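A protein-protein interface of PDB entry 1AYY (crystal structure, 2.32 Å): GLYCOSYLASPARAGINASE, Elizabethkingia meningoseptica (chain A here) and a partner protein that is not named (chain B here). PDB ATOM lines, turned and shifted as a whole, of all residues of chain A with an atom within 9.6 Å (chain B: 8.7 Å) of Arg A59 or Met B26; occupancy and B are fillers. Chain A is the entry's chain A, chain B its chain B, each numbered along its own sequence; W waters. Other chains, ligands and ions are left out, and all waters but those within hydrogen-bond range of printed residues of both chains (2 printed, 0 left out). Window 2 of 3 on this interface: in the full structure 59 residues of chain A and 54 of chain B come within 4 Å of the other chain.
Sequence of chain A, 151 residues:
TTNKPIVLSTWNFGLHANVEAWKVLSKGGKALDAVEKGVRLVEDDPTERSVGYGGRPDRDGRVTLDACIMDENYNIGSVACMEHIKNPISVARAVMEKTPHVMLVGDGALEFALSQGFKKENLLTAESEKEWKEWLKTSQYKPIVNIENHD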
ATOM      1  N   ARG A  56       7.721 -16.325 -23.632  1.00  0.00           N
ATOM      2  CA  ARG A  56       8.097 -17.700 -23.935  1.00  0.00           C
ATOM      3  C   ARG A  56       7.663 -18.577 -22.765  1.00  0.00           C
ATOM      4  O   ARG A  56       7.885 -18.233 -21.605  1.00  0.00           O
ATOM      5  CB  ARG A  56       9.608 -17.794 -24.158  1.00  0.00           C
ATOM      6  CG  ARG A  56      10.113 -16.810 -25.205  1.00  0.00           C
ATOM      7  CD  ARG A  56      11.568 -17.050 -25.565  1.00  0.00           C
ATOM      8  NE  ARG A  56      11.997 -16.167 -26.646  1.00  0.00           N
ATOM      9  CZ  ARG A  56      12.191 -14.859 -26.507  1.00  0.00           C
ATOM     10  NH1 ARG A  56      11.999 -14.278 -25.330  1.00  0.00           N
ATOM     11  NH2 ARG A  56      12.580 -14.131 -27.546  1.00  0.00           N
ATOM     12  N   PRO A  57       7.044 -19.729 -23.060  1.00  0.00           N
ATOM     13  CA  PRO A  57       6.564 -20.660 -22.034  1.00  0.00           C
ATOM     14  C   PRO A  57       7.645 -21.524 -21.403  1.00  0.00           C
ATOM     15  O   PRO A  57       8.817 -21.446 -21.773  1.00  0.00           O
ATOM     16  CB  PRO A  57       5.536 -21.503 -22.780  1.00  0.00           C
ATOM     17  CG  PRO A  57       6.065 -21.549 -24.178  1.00  0.00           C
ATOM     18  CD  PRO A  57       6.779 -20.235 -24.421  1.00  0.00           C
ATOM     19  N   ASP A  58       7.240 -22.344 -20.439  1.00  0.00           N
ATOM     20  CA  ASP A  58       8.168 -23.245 -19.775  1.00  0.00           C
ATOM     21  C   ASP A  58       8.345 -24.468 -20.670  1.00  0.00           C
ATOM     22  O   ASP A  58       7.746 -24.546 -21.742  1.00  0.00           O
ATOM     23  CB  ASP A  58       7.630 -23.656 -18.399  1.00  0.00           C
ATOM     24  CG  ASP A  58       6.242 -24.263 -18.465  1.00  0.00           C
ATOM     25  OD1 ASP A  58       5.874 -24.827 -19.518  1.00  0.00           O
ATOM     26  OD2 ASP A  58       5.517 -24.178 -17.452  1.00  0.00           O
ATOM     27  N   ARG A  59       9.163 -25.421 -20.233  1.00  0.00           N
ATOM     28  CA  ARG A  59       9.416 -26.625 -21.017  1.00  0.00           C
ATOM     29  C   ARG A  59       8.144 -27.389 -21.385  1.00  0.00           C
ATOM     30  O   ARG A  59       8.140 -28.167 -22.340  1.00  0.00           O
ATOM     31  CB  ARG A  59      10.364 -27.552 -20.255  1.00  0.00           C
ATOM     32  CG  ARG A  59       9.975 -27.778 -18.805  1.00  0.00           C
ATOM     33  CD  ARG A  59      10.369 -29.168 -18.334  1.00  0.00           C
ATOM     34  NE  ARG A  59      11.755 -29.486 -18.668  1.00  0.00           N
ATOM     35  CZ  ARG A  59      12.575 -30.174 -17.879  1.00  0.00           C
ATOM     36  NH1 ARG A  59      12.151 -30.623 -16.705  1.00  0.00           N
ATOM     37  NH2 ARG A  59      13.820 -30.416 -18.267  1.00  0.00           N
ATOM     38  N   ASP A  60       7.071 -27.161 -20.636  1.00  0.00           N
ATOM     39  CA  ASP A  60       5.803 -27.844 -20.882  1.00  0.00           C
ATOM     40  C   ASP A  60       4.908 -27.117 -21.879  1.00  0.00           C
ATOM     41  O   ASP A  60       3.887 -27.653 -22.307  1.00  0.00           O
ATOM     42  CB  ASP A  60       5.045 -28.027 -19.565  1.00  0.00           C
ATOM     43  CG  ASP A  60       5.570 -29.189 -18.747  1.00  0.00           C
ATOM     44  OD1 ASP A  60       6.459 -29.914 -19.242  1.00  0.00           O
ATOM     45  OD2 ASP A  60       5.093 -29.378 -17.607  1.00  0.00           O
ATOM     46  N   GLY A  61       5.290 -25.899 -22.246  1.00  0.00           N
ATOM     47  CA  GLY A  61       4.496 -25.132 -23.189  1.00  0.00           C
ATOM     48  C   GLY A  61       3.486 -24.236 -22.499  1.00  0.00           C
ATOM     49  O   GLY A  61       2.565 -23.712 -23.130  1.00  0.00           O
ATOM     50  N   ARG A  62       3.655 -24.064 -21.192  1.00  0.00           N
ATOM     51  CA  ARG A  62       2.761 -23.219 -20.414  1.00  0.00           C
ATOM     52  C   ARG A  62       3.432 -21.881 -20.129  1.00  0.00           C
ATOM     53  O   ARG A  62       4.619 -21.827 -19.806  1.00  0.00           O
ATOM     54  CB  ARG A  62       2.399 -23.905 -19.095  1.00  0.00           C
ATOM     55  CG  ARG A  62       1.642 -25.209 -19.266  1.00  0.00           C
ATOM     56  CD  ARG A  62       1.649 -26.020 -17.984  1.00  0.00           C
ATOM     57  NE  ARG A  62       0.616 -25.579 -17.051  1.00  0.00           N
ATOM     58  CZ  ARG A  62       0.112 -26.339 -16.083  1.00  0.00           C
ATOM     59  NH1 ARG A  62       0.547 -27.581 -15.918  1.00  0.00           N
ATOM     60  NH2 ARG A  62      -0.826 -25.858 -15.278  1.00  0.00           N
ATOM     61  N   VAL A  63       2.668 -20.803 -20.259  1.00  0.00           N
ATOM     62  CA  VAL A  63       3.191 -19.466 -20.009  1.00  0.00           C
ATOM     63  C   VAL A  63       2.820 -19.026 -18.599  1.00  0.00           C
ATOM     64  O   VAL A  63       1.682 -18.637 -18.341  1.00  0.00           O
ATOM     65  CB  VAL A  63       2.625 -18.441 -21.017  1.00  0.00           C
ATOM     66  CG1 VAL A  63       3.098 -17.040 -20.659  1.00  0.00           C
ATOM     67  CG2 VAL A  63       3.066 -18.801 -22.428  1.00  0.00           C
ATOM     68  N   THR A  64       3.784 -19.104 -17.687  1.00  0.00           N
ATOM     69  CA  THR A  64       3.558 -18.709 -16.304  1.00  0.00           C
ATOM     70  C   THR A  64       4.231 -17.366 -16.049  1.00  0.00           C
ATOM     71  O   THR A  64       5.399 -17.170 -16.390  1.00  0.00           O
ATOM     72  CB  THR A  64       4.122 -19.756 -15.323  1.00  0.00           C
ATOM     73  OG1 THR A  64       5.535 -19.890 -15.518  1.00  0.00           O
ATOM     74  CG2 THR A  64       3.454 -21.105 -15.553  1.00  0.00           C
ATOM     75  N   ASP A  66       5.330 -14.057 -13.454  1.00  0.00           N
ATOM     76  CA  ASP A  66       5.718 -13.672 -12.103  1.00  0.00           C
ATOM     77  C   ASP A  66       5.760 -12.151 -12.051  1.00  0.00           C
ATOM     78  O   ASP A  66       6.248 -11.505 -12.979  1.00  0.00           O
ATOM     79  CB  ASP A  66       7.102 -14.224 -11.753  1.00  0.00           C
ATOM     80  CG  ASP A  66       7.241 -15.704 -12.050  1.00  0.00           C
ATOM     81  OD1 ASP A  66       6.218 -16.421 -12.027  1.00  0.00           O
ATOM     82  OD2 ASP A  66       8.381 -16.149 -12.303  1.00  0.00           O
ATOM     83  N   CYS A  81       3.949 -17.821 -10.987  1.00  0.00           N
ATOM     84  CA  CYS A  81       3.447 -18.961 -11.736  1.00  0.00           C
ATOM     85  C   CYS A  81       1.955 -18.844 -12.019  1.00  0.00           C
ATOM     86  O   CYS A  81       1.190 -19.774 -11.760  1.00  0.00           O
ATOM     87  CB  CYS A  81       3.730 -20.259 -10.973  1.00  0.00           C
ATOM     88  SG  CYS A  81       3.941 -21.710 -12.036  1.00  0.00           S
ATOM     89  N   GLU A 129       4.691 -20.411 -29.542  1.00  0.00           N
ATOM     90  CA  GLU A 129       4.371 -21.830 -29.543  1.00  0.00           C
ATOM     91  C   GLU A 129       5.259 -22.562 -30.543  1.00  0.00           C
ATOM     92  O   GLU A 129       5.688 -23.688 -30.298  1.00  0.00           O
ATOM     93  CB  GLU A 129       2.899 -22.038 -29.909  1.00  0.00           C
ATOM     94  CG  GLU A 129       2.487 -23.498 -30.049  1.00  0.00           C
ATOM     95  CD  GLU A 129       1.119 -23.658 -30.686  1.00  0.00           C
ATOM     96  OE1 GLU A 129       0.602 -22.667 -31.242  1.00  0.00           O
ATOM     97  OE2 GLU A 129       0.562 -24.775 -30.630  1.00  0.00           O
ATOM     98  N   TRP A 132       8.857 -22.696 -29.418  1.00  0.00           N
ATOM     99  CA  TRP A 132       8.910 -23.679 -28.344  1.00  0.00           C
ATOM    100  C   TRP A 132       9.096 -25.078 -28.927  1.00  0.00           C
ATOM    101  O   TRP A 132      10.044 -25.784 -28.581  1.00  0.00           O
ATOM    102  CB  TRP A 132       7.622 -23.623 -27.521  1.00  0.00           C
ATOM    103  CG  TRP A 132       7.475 -24.749 -26.542  1.00  0.00           C
ATOM    104  CD1 TRP A 132       8.310 -25.051 -25.505  1.00  0.00           C
ATOM    105  CD2 TRP A 132       6.416 -25.712 -26.500  1.00  0.00           C
ATOM    106  NE1 TRP A 132       7.837 -26.143 -24.817  1.00  0.00           N
ATOM    107  CE2 TRP A 132       6.676 -26.570 -25.406  1.00  0.00           C
ATOM    108  CE3 TRP A 132       5.273 -25.936 -27.279  1.00  0.00           C
ATOM    109  CZ2 TRP A 132       5.833 -27.634 -25.071  1.00  0.00           C
ATOM    110  CZ3 TRP A 132       4.433 -26.995 -26.945  1.00  0.00           C
ATOM    111  CH2 TRP A 132       4.719 -27.831 -25.849  1.00  0.00           C
ATOM    112  N   LYS A 133       8.183 -25.470 -29.811  1.00  0.00           N
ATOM    113  CA  LYS A 133       8.239 -26.781 -30.449  1.00  0.00           C
ATOM    114  C   LYS A 133       9.610 -27.013 -31.072  1.00  0.00           C
ATOM    115  O   LYS A 133      10.152 -28.117 -31.014  1.00  0.00           O
ATOM    116  CB  LYS A 133       7.158 -26.888 -31.527  1.00  0.00           C
ATOM    117  CG  LYS A 133       5.738 -26.829 -30.986  1.00  0.00           C
ATOM    118  CD  LYS A 133       4.781 -27.622 -31.860  1.00  0.00           C
ATOM    119  CE  LYS A 133       3.381 -27.637 -31.270  1.00  0.00           C
ATOM    120  NZ  LYS A 133       2.349 -27.272 -32.281  1.00  0.00           N
ATOM    121  N   TRP A 135      12.395 -25.852 -30.063  1.00  0.00           N
ATOM    122  CA  TRP A 135      13.328 -26.113 -28.975  1.00  0.00           C
ATOM    123  C   TRP A 135      13.186 -27.541 -28.460  1.00  0.00           C
ATOM    124  O   TRP A 135      14.177 -28.196 -28.144  1.00  0.00           O
ATOM    125  CB  TRP A 135      13.079 -25.128 -27.826  1.00  0.00           C
ATOM    126  CG  TRP A 135      13.851 -25.436 -26.576  1.00  0.00           C
ATOM    127  CD1 TRP A 135      15.121 -25.035 -26.277  1.00  0.00           C
ATOM    128  CD2 TRP A 135      13.398 -26.202 -25.452  1.00  0.00           C
ATOM    129  NE1 TRP A 135      15.487 -25.500 -25.037  1.00  0.00           N
ATOM    130  CE2 TRP A 135      14.449 -26.218 -24.508  1.00  0.00           C
ATOM    131  CE3 TRP A 135      12.205 -26.874 -25.148  1.00  0.00           C
ATOM    132  CZ2 TRP A 135      14.343 -26.882 -23.279  1.00  0.00           C
ATOM    133  CZ3 TRP A 135      12.101 -27.533 -23.925  1.00  0.00           C
ATOM    134  CH2 TRP A 135      13.166 -27.532 -23.008  1.00  0.00           C
ATOM    135  N   LEU A 136      11.948 -28.018 -28.380  1.00  0.00           N
ATOM    136  CA  LEU A 136      11.670 -29.366 -27.898  1.00  0.00           C
ATOM    137  C   LEU A 136      12.543 -30.408 -28.587  1.00  0.00           C
ATOM    138  O   LEU A 136      13.007 -31.358 -27.954  1.00  0.00           O
ATOM    139  CB  LEU A 136      10.193 -29.707 -28.115  1.00  0.00           C
ATOM    140  CG  LEU A 136       9.245 -29.370 -26.961  1.00  0.00           C
ATOM    141  CD1 LEU A 136       7.805 -29.555 -27.413  1.00  0.00           C
ATOM    142  CD2 LEU A 136       9.552 -30.261 -25.765  1.00  0.00           C
ATOM    143  N   LYS A 137      12.768 -30.220 -29.884  1.00  0.00           N
ATOM    144  CA  LYS A 137      13.585 -31.138 -30.669  1.00  0.00           C
ATOM    145  C   LYS A 137      14.955 -31.358 -30.036  1.00  0.00           C
ATOM    146  O   LYS A 137      15.332 -32.487 -29.724  1.00  0.00           O
ATOM    147  CB  LYS A 137      13.765 -30.599 -32.091  1.00  0.00           C
ATOM    148  CG  LYS A 137      12.523 -30.700 -32.956  1.00  0.00           C
ATOM    149  CD  LYS A 137      12.637 -31.850 -33.945  1.00  0.00           C
ATOM    150  CE  LYS A 137      11.271 -32.432 -34.275  1.00  0.00           C
ATOM    151  NZ  LYS A 137      11.317 -33.349 -35.450  1.00  0.00           N
ATOM    152  N   SER A 139      15.888 -30.228 -27.115  1.00  0.00           N
ATOM    153  CA  SER A 139      15.718 -30.461 -25.686  1.00  0.00           C
ATOM    154  C   SER A 139      14.258 -30.300 -25.273  1.00  0.00           C
ATOM    155  O   SER A 139      13.655 -31.224 -24.725  1.00  0.00           O
ATOM    156  CB  SER A 139      16.590 -29.492 -24.879  1.00  0.00           C
ATOM    157  OG  SER A 139      16.631 -28.212 -25.487  1.00  0.00           O
ATOM    158  N   MET B  22      12.419 -17.406 -17.166  1.00  0.00           N
ATOM    159  CA  MET B  22      13.381 -17.975 -18.104  1.00  0.00           C
ATOM    160  C   MET B  22      12.633 -18.889 -19.063  1.00  0.00           C
ATOM    161  O   MET B  22      11.856 -19.744 -18.637  1.00  0.00           O
ATOM    162  CB  MET B  22      14.448 -18.779 -17.356  1.00  0.00           C
ATOM    163  CG  MET B  22      15.396 -17.936 -16.518  1.00  0.00           C
ATOM    164  SD  MET B  22      16.257 -16.672 -17.476  1.00  0.00           S
ATOM    165  CE  MET B  22      15.830 -15.211 -16.548  1.00  0.00           C
ATOM    166  N   ALA B  23      12.871 -18.708 -20.357  1.00  0.00           N
ATOM    167  CA  ALA B  23      12.210 -19.511 -21.377  1.00  0.00           C
ATOM    168  C   ALA B  23      12.512 -20.995 -21.222  1.00  0.00           C
ATOM    169  O   ALA B  23      13.644 -21.383 -20.933  1.00  0.00           O
ATOM    170  CB  ALA B  23      12.631 -19.037 -22.767  1.00  0.00           C
ATOM    171  N   TYR B  24      11.488 -21.818 -21.423  1.00  0.00           N
ATOM    172  CA  TYR B  24      11.622 -23.266 -21.329  1.00  0.00           C
ATOM    173  C   TYR B  24      12.126 -23.718 -19.963  1.00  0.00           C
ATOM    174  O   TYR B  24      12.943 -24.632 -19.858  1.00  0.00           O
ATOM    175  CB  TYR B  24      12.557 -23.769 -22.431  1.00  0.00           C
ATOM    176  CG  TYR B  24      12.322 -23.095 -23.766  1.00  0.00           C
ATOM    177  CD1 TYR B  24      11.029 -22.920 -24.260  1.00  0.00           C
ATOM    178  CD2 TYR B  24      13.388 -22.619 -24.526  1.00  0.00           C
ATOM    179  CE1 TYR B  24      10.804 -22.286 -25.479  1.00  0.00           C
ATOM    180  CE2 TYR B  24      13.175 -21.984 -25.747  1.00  0.00           C
ATOM    181  CZ  TYR B  24      11.880 -21.821 -26.216  1.00  0.00           C
ATOM    182  OH  TYR B  24      11.661 -21.193 -27.419  1.00  0.00           O
ATOM    183  N   LYS B  25      11.625 -23.070 -18.919  1.00  0.00           N
ATOM    184  CA  LYS B  25      12.004 -23.402 -17.553  1.00  0.00           C
ATOM    185  C   LYS B  25      11.142 -24.557 -17.056  1.00  0.00           C
ATOM    186  O   LYS B  25      10.155 -24.922 -17.694  1.00  0.00           O
ATOM    187  CB  LYS B  25      11.802 -22.186 -16.645  1.00  0.00           C
ATOM    188  CG  LYS B  25      10.363 -21.985 -16.191  1.00  0.00           C
ATOM    189  CD  LYS B  25       9.933 -20.532 -16.317  1.00  0.00           C
ATOM    190  CE  LYS B  25       8.425 -20.418 -16.490  1.00  0.00           C
ATOM    191  NZ  LYS B  25       7.923 -19.047 -16.198  1.00  0.00           N
ATOM    192  N   MET B  26      11.520 -25.138 -15.923  1.00  0.00           N
ATOM    193  CA  MET B  26      10.746 -26.231 -15.355  1.00  0.00           C
ATOM    194  C   MET B  26       9.392 -25.656 -14.955  1.00  0.00           C
ATOM    195  O   MET B  26       9.320 -24.571 -14.378  1.00  0.00           O
ATOM    196  CB  MET B  26      11.460 -26.816 -14.133  1.00  0.00           C
ATOM    197  CG  MET B  26      12.581 -27.784 -14.482  1.00  0.00           C
ATOM    198  SD  MET B  26      13.623 -28.205 -13.066  1.00  0.00           S
ATOM    199  CE  MET B  26      13.241 -29.943 -12.866  1.00  0.00           C
ATOM    200  N   HIS B  27       8.331 -26.388 -15.273  1.00  0.00           N
ATOM    201  CA  HIS B  27       6.959 -25.974 -14.989  1.00  0.00           C
ATOM    202  C   HIS B  27       6.754 -24.879 -13.940  1.00  0.00           C
ATOM    203  O   HIS B  27       6.534 -23.716 -14.284  1.00  0.00           O
ATOM    204  CB  HIS B  27       6.115 -27.194 -14.609  1.00  0.00           C
ATOM    205  CG  HIS B  27       4.661 -26.884 -14.427  1.00  0.00           C
ATOM    206  ND1 HIS B  27       3.839 -27.621 -13.600  1.00  0.00           N
ATOM    207  CD2 HIS B  27       3.884 -25.908 -14.955  1.00  0.00           C
ATOM    208  CE1 HIS B  27       2.622 -27.111 -13.625  1.00  0.00           C
ATOM    209  NE2 HIS B  27       2.622 -26.070 -14.439  1.00  0.00           N
ATOM    210  N   GLY B  28       6.817 -25.254 -12.666  1.00  0.00           N
ATOM    211  CA  GLY B  28       6.599 -24.286 -11.604  1.00  0.00           C
ATOM    212  C   GLY B  28       7.797 -23.485 -11.131  1.00  0.00           C
ATOM    213  O   GLY B  28       7.853 -23.084  -9.967  1.00  0.00           O
ATOM    214  N   ARG B  29       8.756 -23.241 -12.017  1.00  0.00           N
ATOM    215  CA  ARG B  29       9.938 -22.472 -11.644  1.00  0.00           C
ATOM    216  C   ARG B  29       9.582 -21.005 -11.430  1.00  0.00           C
ATOM    217  O   ARG B  29       8.860 -20.405 -12.230  1.00  0.00           O
ATOM    218  CB  ARG B  29      11.020 -22.575 -12.721  1.00  0.00           C
ATOM    219  CG  ARG B  29      12.283 -21.797 -12.376  1.00  0.00           C
ATOM    220  CD  ARG B  29      12.806 -21.001 -13.562  1.00  0.00           C
ATOM    221  NE  ARG B  29      12.236 -19.659 -13.631  1.00  0.00           N
ATOM    222  CZ  ARG B  29      12.930 -18.536 -13.467  1.00  0.00           C
ATOM    223  NH1 ARG B  29      14.233 -18.583 -13.221  1.00  0.00           N
ATOM    224  NH2 ARG B  29      12.321 -17.362 -13.558  1.00  0.00           N
ATOM    225  N   VAL B  30      10.100 -20.434 -10.348  1.00  0.00           N
ATOM    226  CA  VAL B  30       9.850 -19.037 -10.019  1.00  0.00           C
ATOM    227  C   VAL B  30      11.177 -18.297  -9.888  1.00  0.00           C
ATOM    228  O   VAL B  30      12.104 -18.782  -9.239  1.00  0.00           O
ATOM    229  CB  VAL B  30       9.062 -18.912  -8.693  1.00  0.00           C
ATOM    230  CG1 VAL B  30       9.093 -17.473  -8.196  1.00  0.00           C
ATOM    231  CG2 VAL B  30       7.624 -19.372  -8.902  1.00  0.00           C
ATOM    232  N   GLY B  31      11.260 -17.124 -10.509  1.00  0.00           N
ATOM    233  CA  GLY B  31      12.481 -16.339 -10.454  1.00  0.00           C
ATOM    234  C   GLY B  31      12.508 -15.307  -9.343  1.00  0.00           C
ATOM    235  O   GLY B  31      11.842 -15.459  -8.318  1.00  0.00           O
ATOM    236  N   GLU B  56      17.844 -16.561 -10.506  1.00  0.00           N
ATOM    237  CA  GLU B  56      18.385 -17.494  -9.522  1.00  0.00           C
ATOM    238  C   GLU B  56      19.496 -16.866  -8.686  1.00  0.00           C
ATOM    239  O   GLU B  56      19.578 -17.087  -7.476  1.00  0.00           O
ATOM    240  CB  GLU B  56      18.919 -18.745 -10.222  1.00  0.00           C
ATOM    241  CG  GLU B  56      17.883 -19.844 -10.412  1.00  0.00           C
ATOM    242  CD  GLU B  56      17.013 -19.622 -11.636  1.00  0.00           C
ATOM    243  OE1 GLU B  56      17.290 -18.675 -12.400  1.00  0.00           O
ATOM    244  OE2 GLU B  56      16.049 -20.395 -11.834  1.00  0.00           O
HETATM  245  O   HOH W   1      10.562 -14.518 -11.771  1.00  0.00           O
HETATM  246  O   HOH W   2       9.589 -17.934 -13.839  1.00  0.00           O
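NH1 of Arg A62 lies within hydrogen-bond range of NE2 of His B27 (3.0 Å). NZ of Lys B25 lies within hydrogen-bond range of OG1 of Thr A64, 2.6 Å away. The side-chain carboxylate (OD2) of Asp A58 lies close to the backbone carbonyl oxygen (O) of His B27. The backbone NH (N) of Arg A59 sits at hydrogen-bond distance from the backbone carbonyl oxygen (O) of Lys B25 (2.8 Å). N of Tyr B24 is in hydrogen-bond range of O of Pro A57, 2.7 Å away.
N of Asp A60 is in hydrogen-bond range of OD1 of Asp A58 (2.9 Å). OD1 of Asp A58 lies within hydrogen-bond range of N of Arg A62 (2.9 Å). OD1 of Asp A66 sits at hydrogen-bond distance from N of Cys A81, at 2.9 Å. The side-chain carboxylate of Asp A58 lies within hydrogen-bond range of the backbone NH of Gly A61 (3.0 Å). NE1 of Trp A135 lies within hydrogen-bond range of OG of Ser A139 (3.0 Å). The backbone carbonyl oxygen of Asp A58 sits at hydrogen-bond distance from the indole nitrogen of Trp A132.
CB of Ala B23 touches CB of Arg A56 (3.6 Å). Ala B23 touches Pro A57. C of Asp A58 touches CA of Tyr B24, at 3.6 Å. CB of Asp A58 touches O of Lys B25, at 2.9 Å. C of Tyr B24 touches N of Arg A59, 3.4 Å away. Arg A59 touches Met B26 (NH1 to CG, 3.6 Å). OD2 of Asp A66 touches CA of Val B30, at 3.96 Å. Gly B31 touches Asp A66. Cys A81 touches Gly B28 (SG to CA, 3.7 Å). Tyr B24 touches Trp A135.
Arg A59 touches three residues of chain B. Of the printed residues of chain A, Met B26 touches Arg A59. Printed residues of chain A within 4 Å of His B27: Asp A58, Asp A60, Arg A62 and Cys A81. Printed residues of chain B within 4 Å of Asp A58: Tyr B24, Lys B25 and His B27. Ser A139 touches none of the printed residues of chain B. Leu A136 touches none of the printed residues of chain B.
Of the 18 printed residues of chain A, 11 touch a printed residue of chain B. Hydrophobic or aromatic side chains of chain A within 4 Å of the printed part of chain B: Trp A132 and Trp A135. Of the 11 printed residues of chain B, 8 touch a printed residue of chain A. Hydrophobic or aromatic side chains of chain B that line the printed part of chain A: Ala B23, Tyr B24, Met B26 and His B27. Among the printed residues, 18 pairs touch across the chains. Among the printed residues, no Asp or Glu carboxylate lies within 4 Å of a Lys or Arg side-chain nitrogen of the other chain.
Water W2 lies within hydrogen-bond range of the side-chain carboxylate of Asp A66 (2.6 Å), the guanidinium group of Arg B29 (2.8 Å) and the side-chain amino group of Lys B25 (3.1 Å). Water W1 bridges OD2 of Asp A66 (2.8 Å) and N of Gly B31 (3.0 Å).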
